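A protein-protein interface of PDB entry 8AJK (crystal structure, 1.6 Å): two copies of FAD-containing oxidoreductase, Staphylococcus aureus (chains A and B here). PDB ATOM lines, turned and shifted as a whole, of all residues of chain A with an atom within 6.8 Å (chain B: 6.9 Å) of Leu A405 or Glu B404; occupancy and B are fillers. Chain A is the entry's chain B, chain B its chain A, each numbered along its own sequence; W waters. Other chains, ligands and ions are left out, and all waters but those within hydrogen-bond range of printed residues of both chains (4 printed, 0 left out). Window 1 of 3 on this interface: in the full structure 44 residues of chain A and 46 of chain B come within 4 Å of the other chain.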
ATOM      1  N   SER A 342      14.401  14.912 -24.932  1.00  0.00           N
ATOM      2  CA  SER A 342      14.789  15.263 -23.577  1.00  0.00           C
ATOM      3  C   SER A 342      16.153  15.935 -23.593  1.00  0.00           C
ATOM      4  O   SER A 342      17.012  15.602 -24.417  1.00  0.00           O
ATOM      5  CB  SER A 342      14.809  14.029 -22.674  1.00  0.00           C
ATOM      6  OG  SER A 342      13.527  13.430 -22.632  1.00  0.00           O
ATOM      7  N   ARG A 370      18.263  -2.064 -29.283  1.00  0.00           N
ATOM      8  CA  ARG A 370      16.971  -2.033 -28.590  1.00  0.00           C
ATOM      9  C   ARG A 370      15.857  -1.420 -29.448  1.00  0.00           C
ATOM     10  O   ARG A 370      14.675  -1.748 -29.263  1.00  0.00           O
ATOM     11  CB  ARG A 370      17.103  -1.269 -27.257  1.00  0.00           C
ATOM     12  CG  ARG A 370      15.798  -1.102 -26.451  1.00  0.00           C
ATOM     13  CD  ARG A 370      15.169  -2.414 -25.915  1.00  0.00           C
ATOM     14  NE  ARG A 370      13.731  -2.234 -25.704  1.00  0.00           N
ATOM     15  CZ  ARG A 370      12.994  -2.848 -24.787  1.00  0.00           C
ATOM     16  NH1 ARG A 370      13.514  -3.747 -23.958  1.00  0.00           N
ATOM     17  NH2 ARG A 370      11.691  -2.560 -24.702  1.00  0.00           N
ATOM     18  N   PHE A 381      20.458  10.600 -30.456  1.00  0.00           N
ATOM     19  CA  PHE A 381      21.060  10.941 -29.173  1.00  0.00           C
ATOM     20  C   PHE A 381      22.338  11.728 -29.420  1.00  0.00           C
ATOM     21  O   PHE A 381      23.157  11.348 -30.259  1.00  0.00           O
ATOM     22  CB  PHE A 381      21.392   9.690 -28.348  1.00  0.00           C
ATOM     23  CG  PHE A 381      20.190   8.965 -27.772  1.00  0.00           C
ATOM     24  CD1 PHE A 381      18.887   9.414 -27.979  1.00  0.00           C
ATOM     25  CD2 PHE A 381      20.386   7.827 -26.990  1.00  0.00           C
ATOM     26  CE1 PHE A 381      17.799   8.717 -27.432  1.00  0.00           C
ATOM     27  CE2 PHE A 381      19.307   7.143 -26.430  1.00  0.00           C
ATOM     28  CZ  PHE A 381      18.019   7.584 -26.645  1.00  0.00           C
ATOM     29  N   LEU A 397      18.577  13.813 -25.830  1.00  0.00           N
ATOM     30  CA  LEU A 397      18.167  12.430 -26.120  1.00  0.00           C
ATOM     31  C   LEU A 397      16.783  12.489 -26.759  1.00  0.00           C
ATOM     32  O   LEU A 397      15.780  12.715 -26.076  1.00  0.00           O
ATOM     33  CB  LEU A 397      18.162  11.572 -24.851  1.00  0.00           C
ATOM     34  CG  LEU A 397      19.450  11.595 -24.014  1.00  0.00           C
ATOM     35  CD1 LEU A 397      19.257  10.751 -22.754  1.00  0.00           C
ATOM     36  CD2 LEU A 397      20.654  11.086 -24.828  1.00  0.00           C
ATOM     37  N   GLY A 399      14.219  10.264 -28.540  1.00  0.00           N
ATOM     38  CA  GLY A 399      13.963   8.849 -28.766  1.00  0.00           C
ATOM     39  C   GLY A 399      13.250   8.224 -27.588  1.00  0.00           C
ATOM     40  O   GLY A 399      13.138   8.807 -26.520  1.00  0.00           O
ATOM     41  N   LYS A 400      12.760   6.994 -27.801  1.00  0.00           N
ATOM     42  CA  LYS A 400      12.023   6.297 -26.747  1.00  0.00           C
ATOM     43  C   LYS A 400      12.849   6.157 -25.472  1.00  0.00           C
ATOM     44  O   LYS A 400      14.063   5.943 -25.516  1.00  0.00           O
ATOM     45  CB  LYS A 400      11.578   4.915 -27.246  1.00  0.00           C
ATOM     46  CG  LYS A 400      10.254   4.981 -28.048  1.00  0.00           C
ATOM     47  CD  LYS A 400       9.683   3.560 -28.202  1.00  0.00           C
ATOM     48  CE  LYS A 400       8.676   3.405 -29.325  1.00  0.00           C
ATOM     49  NZ  LYS A 400       7.949   4.638 -29.759  1.00  0.00           N
ATOM     50  N   GLN A 401      12.170   6.308 -24.327  1.00  0.00           N
ATOM     51  CA  GLN A 401      12.687   6.238 -22.962  1.00  0.00           C
ATOM     52  C   GLN A 401      13.522   7.451 -22.561  1.00  0.00           C
ATOM     53  O   GLN A 401      14.076   7.466 -21.458  1.00  0.00           O
ATOM     54  CB  GLN A 401      13.506   4.960 -22.707  1.00  0.00           C
ATOM     55  CG  GLN A 401      12.776   3.646 -23.104  1.00  0.00           C
ATOM     56  CD  GLN A 401      11.566   3.313 -22.226  1.00  0.00           C
ATOM     57  OE1 GLN A 401      10.588   4.057 -22.190  1.00  0.00           O
ATOM     58  NE2 GLN A 401      11.614   2.157 -21.544  1.00  0.00           N
ATOM     59  N   SER A 402      13.607   8.487 -23.402  1.00  0.00           N
ATOM     60  CA  SER A 402      14.494   9.601 -23.084  1.00  0.00           C
ATOM     61  C   SER A 402      14.045  10.348 -21.837  1.00  0.00           C
ATOM     62  O   SER A 402      14.893  10.874 -21.098  1.00  0.00           O
ATOM     63  CB  SER A 402      14.613  10.554 -24.273  1.00  0.00           C
ATOM     64  OG  SER A 402      13.411  11.314 -24.468  1.00  0.00           O
ATOM     65  N   GLU A 403      12.738  10.369 -21.553  1.00  0.00           N
ATOM     66  CA  GLU A 403      12.284  11.086 -20.366  1.00  0.00           C
ATOM     67  C   GLU A 403      12.749  10.394 -19.087  1.00  0.00           C
ATOM     68  O   GLU A 403      12.850  11.045 -18.038  1.00  0.00           O
ATOM     69  CB  GLU A 403      10.756  11.255 -20.392  1.00  0.00           C
ATOM     70  CG  GLU A 403       9.930  10.025 -19.978  1.00  0.00           C
ATOM     71  CD  GLU A 403       9.606   9.060 -21.134  1.00  0.00           C
ATOM     72  OE1 GLU A 403      10.332   9.051 -22.155  1.00  0.00           O
ATOM     73  OE2 GLU A 403       8.615   8.303 -21.007  1.00  0.00           O
ATOM     74  N   GLU A 404      13.074   9.104 -19.159  1.00  0.00           N
ATOM     75  CA  GLU A 404      13.700   8.429 -18.026  1.00  0.00           C
ATOM     76  C   GLU A 404      15.224   8.557 -18.078  1.00  0.00           C
ATOM     77  O   GLU A 404      15.854   8.890 -17.069  1.00  0.00           O
ATOM     78  CB  GLU A 404      13.287   6.935 -18.003  1.00  0.00           C
ATOM     79  CG  GLU A 404      11.755   6.690 -18.023  1.00  0.00           C
ATOM     80  CD  GLU A 404      11.015   7.170 -16.765  1.00  0.00           C
ATOM     81  OE1 GLU A 404      11.666   7.549 -15.770  1.00  0.00           O
ATOM     82  OE2 GLU A 404       9.763   7.152 -16.774  1.00  0.00           O
ATOM     83  N   LEU A 405      15.832   8.301 -19.246  1.00  0.00           N
ATOM     84  CA  LEU A 405      17.302   8.266 -19.339  1.00  0.00           C
ATOM     85  C   LEU A 405      17.957   9.613 -19.030  1.00  0.00           C
ATOM     86  O   LEU A 405      19.092   9.653 -18.533  1.00  0.00           O
ATOM     87  CB  LEU A 405      17.735   7.849 -20.735  1.00  0.00           C
ATOM     88  CG  LEU A 405      17.385   6.439 -21.217  1.00  0.00           C
ATOM     89  CD1 LEU A 405      17.956   6.275 -22.611  1.00  0.00           C
ATOM     90  CD2 LEU A 405      17.923   5.394 -20.268  1.00  0.00           C
ATOM     91  N   ILE A 406      17.306  10.725 -19.382  1.00  0.00           N
ATOM     92  CA  ILE A 406      17.956  12.020 -19.208  1.00  0.00           C
ATOM     93  C   ILE A 406      18.341  12.249 -17.753  1.00  0.00           C
ATOM     94  O   ILE A 406      19.304  12.971 -17.470  1.00  0.00           O
ATOM     95  CB  ILE A 406      17.051  13.157 -19.754  1.00  0.00           C
ATOM     96  CG1 ILE A 406      17.879  14.431 -19.987  1.00  0.00           C
ATOM     97  CG2 ILE A 406      15.860  13.437 -18.817  1.00  0.00           C
ATOM     98  CD1 ILE A 406      18.725  14.360 -21.253  1.00  0.00           C
ATOM     99  N   ASN A 407      17.637  11.610 -16.823  1.00  0.00           N
ATOM    100  CA  ASN A 407      17.945  11.751 -15.407  1.00  0.00           C
ATOM    101  C   ASN A 407      19.298  11.145 -15.037  1.00  0.00           C
ATOM    102  O   ASN A 407      19.916  11.583 -14.060  1.00  0.00           O
ATOM    103  CB  ASN A 407      16.818  11.120 -14.578  1.00  0.00           C
ATOM    104  CG  ASN A 407      15.491  11.836 -14.784  1.00  0.00           C
ATOM    105  OD1 ASN A 407      15.312  12.965 -14.322  1.00  0.00           O
ATOM    106  ND2 ASN A 407      14.561  11.195 -15.513  1.00  0.00           N
ATOM    107  N   ILE A 408      19.780  10.153 -15.796  1.00  0.00           N
ATOM    108  CA  ILE A 408      21.118   9.621 -15.534  1.00  0.00           C
ATOM    109  C   ILE A 408      22.154  10.689 -15.831  1.00  0.00           C
ATOM    110  O   ILE A 408      23.122  10.863 -15.085  1.00  0.00           O
ATOM    111  CB  ILE A 408      21.386   8.359 -16.374  1.00  0.00           C
ATOM    112  CG1 ILE A 408      20.419   7.247 -16.023  1.00  0.00           C
ATOM    113  CG2 ILE A 408      22.845   7.886 -16.189  1.00  0.00           C
ATOM    114  CD1 ILE A 408      20.410   6.120 -17.081  1.00  0.00           C
ATOM    115  N   ILE A 409      21.953  11.427 -16.923  1.00  0.00           N
ATOM    116  CA  ILE A 409      22.931  12.421 -17.344  1.00  0.00           C
ATOM    117  C   ILE A 409      22.879  13.637 -16.428  1.00  0.00           C
ATOM    118  O   ILE A 409      23.925  14.206 -16.079  1.00  0.00           O
ATOM    119  CB  ILE A 409      22.718  12.779 -18.828  1.00  0.00           C
ATOM    120  CG1 ILE A 409      22.995  11.524 -19.679  1.00  0.00           C
ATOM    121  CG2 ILE A 409      23.627  13.902 -19.268  1.00  0.00           C
ATOM    122  CD1 ILE A 409      22.752  11.746 -21.176  1.00  0.00           C
ATOM    123  N   LYS A 410      21.673  14.037 -15.998  1.00  0.00           N
ATOM    124  CA  LYS A 410      21.556  15.081 -14.974  1.00  0.00           C
ATOM    125  C   LYS A 410      22.371  14.732 -13.732  1.00  0.00           C
ATOM    126  O   LYS A 410      23.114  15.570 -13.199  1.00  0.00           O
ATOM    127  CB  LYS A 410      20.076  15.289 -14.604  1.00  0.00           C
ATOM    128  CG  LYS A 410      19.769  16.378 -13.538  1.00  0.00           C
ATOM    129  CD  LYS A 410      19.957  15.856 -12.082  1.00  0.00           C
ATOM    130  CE  LYS A 410      19.179  16.700 -11.070  1.00  0.00           C
ATOM    131  NZ  LYS A 410      19.686  18.108 -10.974  1.00  0.00           N
ATOM    132  N   THR A 428      22.013  -2.717 -17.825  1.00  0.00           N
ATOM    133  CA  THR A 428      21.117  -3.827 -18.130  1.00  0.00           C
ATOM    134  C   THR A 428      20.889  -3.908 -19.644  1.00  0.00           C
ATOM    135  O   THR A 428      21.213  -2.988 -20.407  1.00  0.00           O
ATOM    136  CB  THR A 428      19.796  -3.675 -17.369  1.00  0.00           C
ATOM    137  OG1 THR A 428      19.343  -2.321 -17.471  1.00  0.00           O
ATOM    138  CG2 THR A 428      19.989  -4.021 -15.878  1.00  0.00           C
ATOM    139  N   PRO A 430      18.284  -6.167 -22.745  1.00  0.00           N
ATOM    140  CA  PRO A 430      18.381  -5.133 -23.792  1.00  0.00           C
ATOM    141  C   PRO A 430      17.584  -3.889 -23.413  1.00  0.00           C
ATOM    142  O   PRO A 430      16.401  -3.968 -23.087  1.00  0.00           O
ATOM    143  CB  PRO A 430      17.802  -5.838 -25.026  1.00  0.00           C
ATOM    144  CG  PRO A 430      16.813  -6.848 -24.465  1.00  0.00           C
ATOM    145  CD  PRO A 430      17.257  -7.181 -23.055  1.00  0.00           C
ATOM    146  N   THR A 431      18.232  -2.723 -23.435  1.00  0.00           N
ATOM    147  CA  THR A 431      17.637  -1.487 -22.916  1.00  0.00           C
ATOM    148  C   THR A 431      18.038  -0.326 -23.809  1.00  0.00           C
ATOM    149  O   THR A 431      18.902  -0.451 -24.676  1.00  0.00           O
ATOM    150  CB  THR A 431      18.103  -1.185 -21.481  1.00  0.00           C
ATOM    151  OG1 THR A 431      19.527  -0.986 -21.471  1.00  0.00           O
ATOM    152  CG2 THR A 431      17.760  -2.328 -20.503  1.00  0.00           C
ATOM    153  N   MET A 432      17.406   0.830 -23.583  1.00  0.00           N
ATOM    154  CA  MET A 432      17.936   2.038 -24.202  1.00  0.00           C
ATOM    155  C   MET A 432      19.152   2.576 -23.436  1.00  0.00           C
ATOM    156  O   MET A 432      20.044   3.167 -24.046  1.00  0.00           O
ATOM    157  CB  MET A 432      16.836   3.121 -24.272  1.00  0.00           C
ATOM    158  CG  MET A 432      15.682   2.676 -25.146  1.00  0.00           C
ATOM    159  SD  MET A 432      16.068   2.461 -26.910  1.00  0.00           S
ATOM    160  CE  MET A 432      16.310   4.181 -27.511  1.00  0.00           C
ATOM    161  N   ALA A 433      19.196   2.381 -22.123  1.00  0.00           N
ATOM    162  CA  ALA A 433      20.286   2.922 -21.316  1.00  0.00           C
ATOM    163  C   ALA A 433      21.646   2.411 -21.779  1.00  0.00           C
ATOM    164  O   ALA A 433      22.630   3.162 -21.806  1.00  0.00           O
ATOM    165  CB  ALA A 433      20.087   2.548 -19.839  1.00  0.00           C
ATOM    166  N   GLU A 434      21.713   1.142 -22.190  1.00  0.00           N
ATOM    167  CA  GLU A 434      22.998   0.578 -22.595  1.00  0.00           C
ATOM    168  C   GLU A 434      23.561   1.236 -23.853  1.00  0.00           C
ATOM    169  O   GLU A 434      24.746   1.054 -24.158  1.00  0.00           O
ATOM    170  CB  GLU A 434      22.862  -0.939 -22.792  1.00  0.00           C
ATOM    171  CG  GLU A 434      21.977  -1.328 -23.974  1.00  0.00           C
ATOM    172  CD  GLU A 434      21.858  -2.834 -24.129  1.00  0.00           C
ATOM    173  OE1 GLU A 434      22.840  -3.542 -23.847  1.00  0.00           O
ATOM    174  OE2 GLU A 434      20.793  -3.298 -24.574  1.00  0.00           O
ATOM    175  N   SER A 435      22.765   2.030 -24.567  1.00  0.00           N
ATOM    176  CA  SER A 435      23.301   2.768 -25.702  1.00  0.00           C
ATOM    177  C   SER A 435      24.375   3.748 -25.261  1.00  0.00           C
ATOM    178  O   SER A 435      25.155   4.212 -26.103  1.00  0.00           O
ATOM    179  CB  SER A 435      22.173   3.524 -26.426  1.00  0.00           C
ATOM    180  OG  SER A 435      21.726   4.622 -25.638  1.00  0.00           O
ATOM    181  N   PHE A 436      24.441   4.041 -23.961  1.00  0.00           N
ATOM    182  CA  PHE A 436      25.462   4.952 -23.450  1.00  0.00           C
ATOM    183  C   PHE A 436      26.860   4.384 -23.661  1.00  0.00           C
ATOM    184  O   PHE A 436      27.824   5.150 -23.774  1.00  0.00           O
ATOM    185  CB  PHE A 436      25.232   5.229 -21.954  1.00  0.00           C
ATOM    186  CG  PHE A 436      24.106   6.208 -21.662  1.00  0.00           C
ATOM    187  CD1 PHE A 436      23.262   6.670 -22.670  1.00  0.00           C
ATOM    188  CD2 PHE A 436      23.888   6.653 -20.366  1.00  0.00           C
ATOM    189  CE1 PHE A 436      22.218   7.565 -22.375  1.00  0.00           C
ATOM    190  CE2 PHE A 436      22.867   7.547 -20.061  1.00  0.00           C
ATOM    191  CZ  PHE A 436      22.016   8.006 -21.074  1.00  0.00           C
ATOM    192  N   THR B 334      17.798  -7.714 -14.641  1.00  0.00           N
ATOM    193  CA  THR B 334      16.367  -7.554 -14.841  1.00  0.00           C
ATOM    194  C   THR B 334      15.773  -8.917 -15.136  1.00  0.00           C
ATOM    195  O   THR B 334      16.296  -9.650 -15.983  1.00  0.00           O
ATOM    196  CB  THR B 334      16.063  -6.589 -15.991  1.00  0.00           C
ATOM    197  OG1 THR B 334      16.457  -5.257 -15.637  1.00  0.00           O
ATOM    198  CG2 THR B 334      14.556  -6.595 -16.301  1.00  0.00           C
ATOM    199  N   SER B 342      13.648  -5.518 -11.578  1.00  0.00           N
ATOM    200  CA  SER B 342      15.053  -5.170 -11.740  1.00  0.00           C
ATOM    201  C   SER B 342      15.731  -5.049 -10.378  1.00  0.00           C
ATOM    202  O   SER B 342      15.111  -4.671  -9.381  1.00  0.00           O
ATOM    203  CB  SER B 342      15.195  -3.858 -12.534  1.00  0.00           C
ATOM    204  OG  SER B 342      14.591  -4.001 -13.815  1.00  0.00           O
ATOM    205  N   LEU B 397      13.464  -2.950  -8.018  1.00  0.00           N
ATOM    206  CA  LEU B 397      12.428  -2.137  -8.656  1.00  0.00           C
ATOM    207  C   LEU B 397      11.556  -3.055  -9.501  1.00  0.00           C
ATOM    208  O   LEU B 397      11.956  -3.467 -10.590  1.00  0.00           O
ATOM    209  CB  LEU B 397      13.033  -1.018  -9.510  1.00  0.00           C
ATOM    210  CG  LEU B 397      14.042  -0.093  -8.843  1.00  0.00           C
ATOM    211  CD1 LEU B 397      14.534   0.901  -9.876  1.00  0.00           C
ATOM    212  CD2 LEU B 397      13.423   0.608  -7.636  1.00  0.00           C
ATOM    213  N   GLN B 401       9.344   0.427 -16.512  1.00  0.00           N
ATOM    214  CA  GLN B 401      10.567   1.199 -16.728  1.00  0.00           C
ATOM    215  C   GLN B 401      11.705   0.791 -15.804  1.00  0.00           C
ATOM    216  O   GLN B 401      12.752   1.441 -15.817  1.00  0.00           O
ATOM    217  CB  GLN B 401      10.347   2.720 -16.589  1.00  0.00           C
ATOM    218  CG  GLN B 401       9.167   3.240 -17.425  1.00  0.00           C
ATOM    219  CD  GLN B 401       9.435   3.175 -18.919  1.00  0.00           C
ATOM    220  OE1 GLN B 401       9.515   2.096 -19.499  1.00  0.00           O
ATOM    221  NE2 GLN B 401       9.507   4.345 -19.565  1.00  0.00           N
ATOM    222  N   SER B 402      11.542  -0.277 -15.016  1.00  0.00           N
ATOM    223  CA  SER B 402      12.568  -0.604 -14.030  1.00  0.00           C
ATOM    224  C   SER B 402      13.868  -1.015 -14.694  1.00  0.00           C
ATOM    225  O   SER B 402      14.945  -0.821 -14.113  1.00  0.00           O
ATOM    226  CB  SER B 402      12.095  -1.722 -13.096  1.00  0.00           C
ATOM    227  OG  SER B 402      12.063  -2.968 -13.777  1.00  0.00           O
ATOM    228  N   GLU B 403      13.798  -1.583 -15.898  1.00  0.00           N
ATOM    229  CA  GLU B 403      15.023  -1.984 -16.570  1.00  0.00           C
ATOM    230  C   GLU B 403      15.866  -0.789 -16.985  1.00  0.00           C
ATOM    231  O   GLU B 403      17.086  -0.940 -17.147  1.00  0.00           O
ATOM    232  CB  GLU B 403      14.713  -2.895 -17.765  1.00  0.00           C
ATOM    233  CG  GLU B 403      14.205  -2.203 -19.061  1.00  0.00           C
ATOM    234  CD  GLU B 403      12.687  -1.986 -19.135  1.00  0.00           C
ATOM    235  OE1 GLU B 403      12.000  -1.948 -18.084  1.00  0.00           O
ATOM    236  OE2 GLU B 403      12.187  -1.844 -20.283  1.00  0.00           O
ATOM    237  N   GLU B 404      15.262   0.398 -17.129  1.00  0.00           N
ATOM    238  CA  GLU B 404      16.049   1.615 -17.302  1.00  0.00           C
ATOM    239  C   GLU B 404      16.417   2.253 -15.970  1.00  0.00           C
ATOM    240  O   GLU B 404      17.568   2.674 -15.782  1.00  0.00           O
ATOM    241  CB  GLU B 404      15.280   2.635 -18.164  1.00  0.00           C
ATOM    242  CG  GLU B 404      14.735   2.081 -19.493  1.00  0.00           C
ATOM    243  CD  GLU B 404      15.788   1.712 -20.530  1.00  0.00           C
ATOM    244  OE1 GLU B 404      16.970   2.050 -20.351  1.00  0.00           O
ATOM    245  OE2 GLU B 404      15.405   1.107 -21.571  1.00  0.00           O
ATOM    246  N   LEU B 405      15.460   2.328 -15.037  1.00  0.00           N
ATOM    247  CA  LEU B 405      15.696   3.039 -13.783  1.00  0.00           C
ATOM    248  C   LEU B 405      16.791   2.394 -12.950  1.00  0.00           C
ATOM    249  O   LEU B 405      17.507   3.101 -12.223  1.00  0.00           O
ATOM    250  CB  LEU B 405      14.427   3.104 -12.933  1.00  0.00           C
ATOM    251  CG  LEU B 405      13.248   3.902 -13.483  1.00  0.00           C
ATOM    252  CD1 LEU B 405      12.142   3.951 -12.440  1.00  0.00           C
ATOM    253  CD2 LEU B 405      13.685   5.304 -13.896  1.00  0.00           C
ATOM    254  N   ILE B 406      16.894   1.060 -12.980  1.00  0.00           N
ATOM    255  CA  ILE B 406      17.870   0.402 -12.108  1.00  0.00           C
ATOM    256  C   ILE B 406      19.284   0.908 -12.384  1.00  0.00           C
ATOM    257  O   ILE B 406      20.133   0.884 -11.488  1.00  0.00           O
ATOM    258  CB  ILE B 406      17.752  -1.142 -12.242  1.00  0.00           C
ATOM    259  CG1 ILE B 406      18.358  -1.873 -11.023  1.00  0.00           C
ATOM    260  CG2 ILE B 406      18.401  -1.640 -13.524  1.00  0.00           C
ATOM    261  CD1 ILE B 406      17.540  -1.676  -9.748  1.00  0.00           C
ATOM    262  N   ASN B 407      19.542   1.432 -13.589  1.00  0.00           N
ATOM    263  CA  ASN B 407      20.876   1.940 -13.909  1.00  0.00           C
ATOM    264  C   ASN B 407      21.207   3.214 -13.154  1.00  0.00           C
ATOM    265  O   ASN B 407      22.389   3.496 -12.915  1.00  0.00           O
ATOM    266  CB  ASN B 407      21.000   2.169 -15.414  1.00  0.00           C
ATOM    267  CG  ASN B 407      20.843   0.891 -16.190  1.00  0.00           C
ATOM    268  OD1 ASN B 407      21.705   0.010 -16.137  1.00  0.00           O
ATOM    269  ND2 ASN B 407      19.721   0.745 -16.873  1.00  0.00           N
ATOM    270  N   ILE B 408      20.194   3.992 -12.765  1.00  0.00           N
ATOM    271  CA  ILE B 408      20.466   5.161 -11.929  1.00  0.00           C
ATOM    272  C   ILE B 408      21.039   4.720 -10.596  1.00  0.00           C
ATOM    273  O   ILE B 408      21.977   5.326 -10.069  1.00  0.00           O
ATOM    274  CB  ILE B 408      19.192   5.989 -11.710  1.00  0.00           C
ATOM    275  CG1 ILE B 408      18.745   6.646 -13.009  1.00  0.00           C
ATOM    276  CG2 ILE B 408      19.469   7.089 -10.685  1.00  0.00           C
ATOM    277  CD1 ILE B 408      17.277   7.034 -12.991  1.00  0.00           C
ATOM    278  N   ILE B 409      20.452   3.677 -10.013  1.00  0.00           N
ATOM    279  CA  ILE B 409      20.869   3.238  -8.690  1.00  0.00           C
ATOM    280  C   ILE B 409      22.217   2.538  -8.758  1.00  0.00           C
ATOM    281  O   ILE B 409      23.051   2.688  -7.852  1.00  0.00           O
ATOM    282  CB  ILE B 409      19.778   2.351  -8.066  1.00  0.00           C
ATOM    283  CG1 ILE B 409      18.499   3.187  -7.911  1.00  0.00           C
ATOM    284  CG2 ILE B 409      20.230   1.806  -6.701  1.00  0.00           C
ATOM    285  CD1 ILE B 409      17.291   2.418  -7.474  1.00  0.00           C
ATOM    286  N   THR B 428      12.657  14.699 -14.201  1.00  0.00           N
ATOM    287  CA  THR B 428      11.628  15.060 -15.174  1.00  0.00           C
ATOM    288  C   THR B 428      10.276  14.513 -14.716  1.00  0.00           C
ATOM    289  O   THR B 428      10.188  13.652 -13.843  1.00  0.00           O
ATOM    290  CB  THR B 428      11.966  14.523 -16.565  1.00  0.00           C
ATOM    291  OG1 THR B 428      12.409  13.177 -16.428  1.00  0.00           O
ATOM    292  CG2 THR B 428      13.084  15.348 -17.208  1.00  0.00           C
ATOM    293  N   ALA B 433      10.910   7.837 -12.982  1.00  0.00           N
ATOM    294  CA  ALA B 433      12.116   8.208 -12.254  1.00  0.00           C
ATOM    295  C   ALA B 433      11.812   9.149 -11.093  1.00  0.00           C
ATOM    296  O   ALA B 433      12.453   9.057 -10.038  1.00  0.00           O
ATOM    297  CB  ALA B 433      13.132   8.857 -13.197  1.00  0.00           C
HETATM  298  O   HOH W   1       9.820  -0.499 -20.959  1.00  0.00           O
HETATM  299  O   HOH W   2      13.247  -0.124 -22.361  1.00  0.00           O
HETATM  300  O   HOH W   3       8.125   5.803 -22.187  1.00  0.00           O
HETATM  301  O   HOH W   4       8.048   6.931 -18.624  1.00  0.00           O
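NE2 of Gln B401 sits at hydrogen-bond distance from OE1 of Gln A401 (2.9 Å). The backbone carbonyl oxygen (O) of Glu B403 lies within hydrogen-bond range of the side-chain hydroxyl (OG1) of Thr A428 (2.7 Å). The backbone NH (N) of Met A432 is in hydrogen-bond range of the side-chain carboxylate (OE2) of Glu B404, at 2.9 Å. OE1 of Glu B404 is in hydrogen-bond range of N of Ala A433 (2.9 Å). The side-chain amide nitrogen of Asn B407 is in hydrogen-bond range of the side-chain hydroxyl of Thr A428. The side-chain hydroxyl (OG1) of Thr B428 lies within hydrogen-bond range of the backbone carbonyl oxygen (O) of Glu A403, at 2.7 Å. The side-chain hydroxyl (OG1) of Thr B428 sits at hydrogen-bond distance from the side-chain amide nitrogen (ND2) of Asn A407. The side-chain carboxylate of Glu A404 lies within hydrogen-bond range of the backbone NH of Ala B433, at 2.9 Å.
The side-chain hydroxyl of Ser B342 is in hydrogen-bond range of the side-chain hydroxyl of Thr B334, at 2.9 Å. The side-chain amide nitrogen (ND2) of Asn B407 is in hydrogen-bond range of the backbone carbonyl oxygen (O) of Glu B404 (3.1 Å). O of Glu A403 is in hydrogen-bond range of ND2 of Asn A407. OG1 of Thr A431 is in hydrogen-bond range of O of Thr A428. OG1 of Thr A431 lies close to N of Ala A433 (3.4 Å).
Among the printed residues, merely in contact across the chains: Gln A401 with Glu B404, Glu A404 with Gln B401, Glu A404 with Leu B405, Leu A405 with Glu B404, Ile A406 with Thr B428, Asn A407 with Ala B433, Ile A408 with Ile B408, Thr A428 with Thr B334, Thr A428 with Ile B406, Thr A431 with Glu B403, Thr A431 with Glu B404 and Ala A433 with Asn B407.
Ser A342 touches none of the printed residues of chain B. Printed residues of chain B within 4 Å of Ile A406: Thr B428 (3.7 Å). Printed residues of chain B within 4 Å of Ile A408: Ile B408 (3.5 Å). Of the printed residues of chain B, Met A432 touches Glu B404 (2.9 Å). Glu B404 touches just these residues of chain A: Gln A401 (3.7 Å), Leu A405 (3.5 Å), Thr A431 (3.5 Å), Met A432 (2.9 Å) and Ala A433 (2.9 Å). The nearest residue of chain B that does not touch Leu A405 is Asn B407 (6.0 Å). The nearest residue of chain A that does not touch Glu B404 is Ile A408 (4.7 Å). The nearest printed residue of chain B that does not touch Thr A428 is Glu B404 (4.9 Å).
Of the 24 printed residues of chain A, 11 touch a printed residue of chain B. Along chain A the printed residues that touch a printed residue of chain B span positions 401 to 433. Printed residues of chain B that touch a printed residue of chain A: Thr B334, Gln B401, Glu B403, Glu B404, Leu B405, Ile B406, Asn B407, Ile B408, Thr B428 and Ala B433. Hydrophobic or aromatic side chains of chain B that line the printed part of chain A: Leu B405, Ile B406, Ile B408 and Ala B433.
Gln A401 touches its own counterpart, Gln B401. Gln A401 touches Glu B404, and with the chains exchanged Glu A404 touches Gln B401. Ile A406 touches Thr B428, and with the chains exchanged Thr A428 touches Ile B406. Positions printed for both chains: 342, 397, 401, 402, 403, 404, 405, 406, 407, 408, 409, 428 and 433. Of the 20 pairs that touch across the chains among the printed residues, 16 have their exchanged pair printed and touching as well.
Water W4 lies within hydrogen-bond range of the side-chain carboxylate of Glu A404 (2.5 Å), the side-chain carboxylate of Glu A403 (2.8 Å) and the side-chain amide nitrogen of Gln B401 (3.1 Å). Water W1 lies within hydrogen-bond range of OE2 of Glu B403, OE1 of Gln B401 and NE2 of Gln A401.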
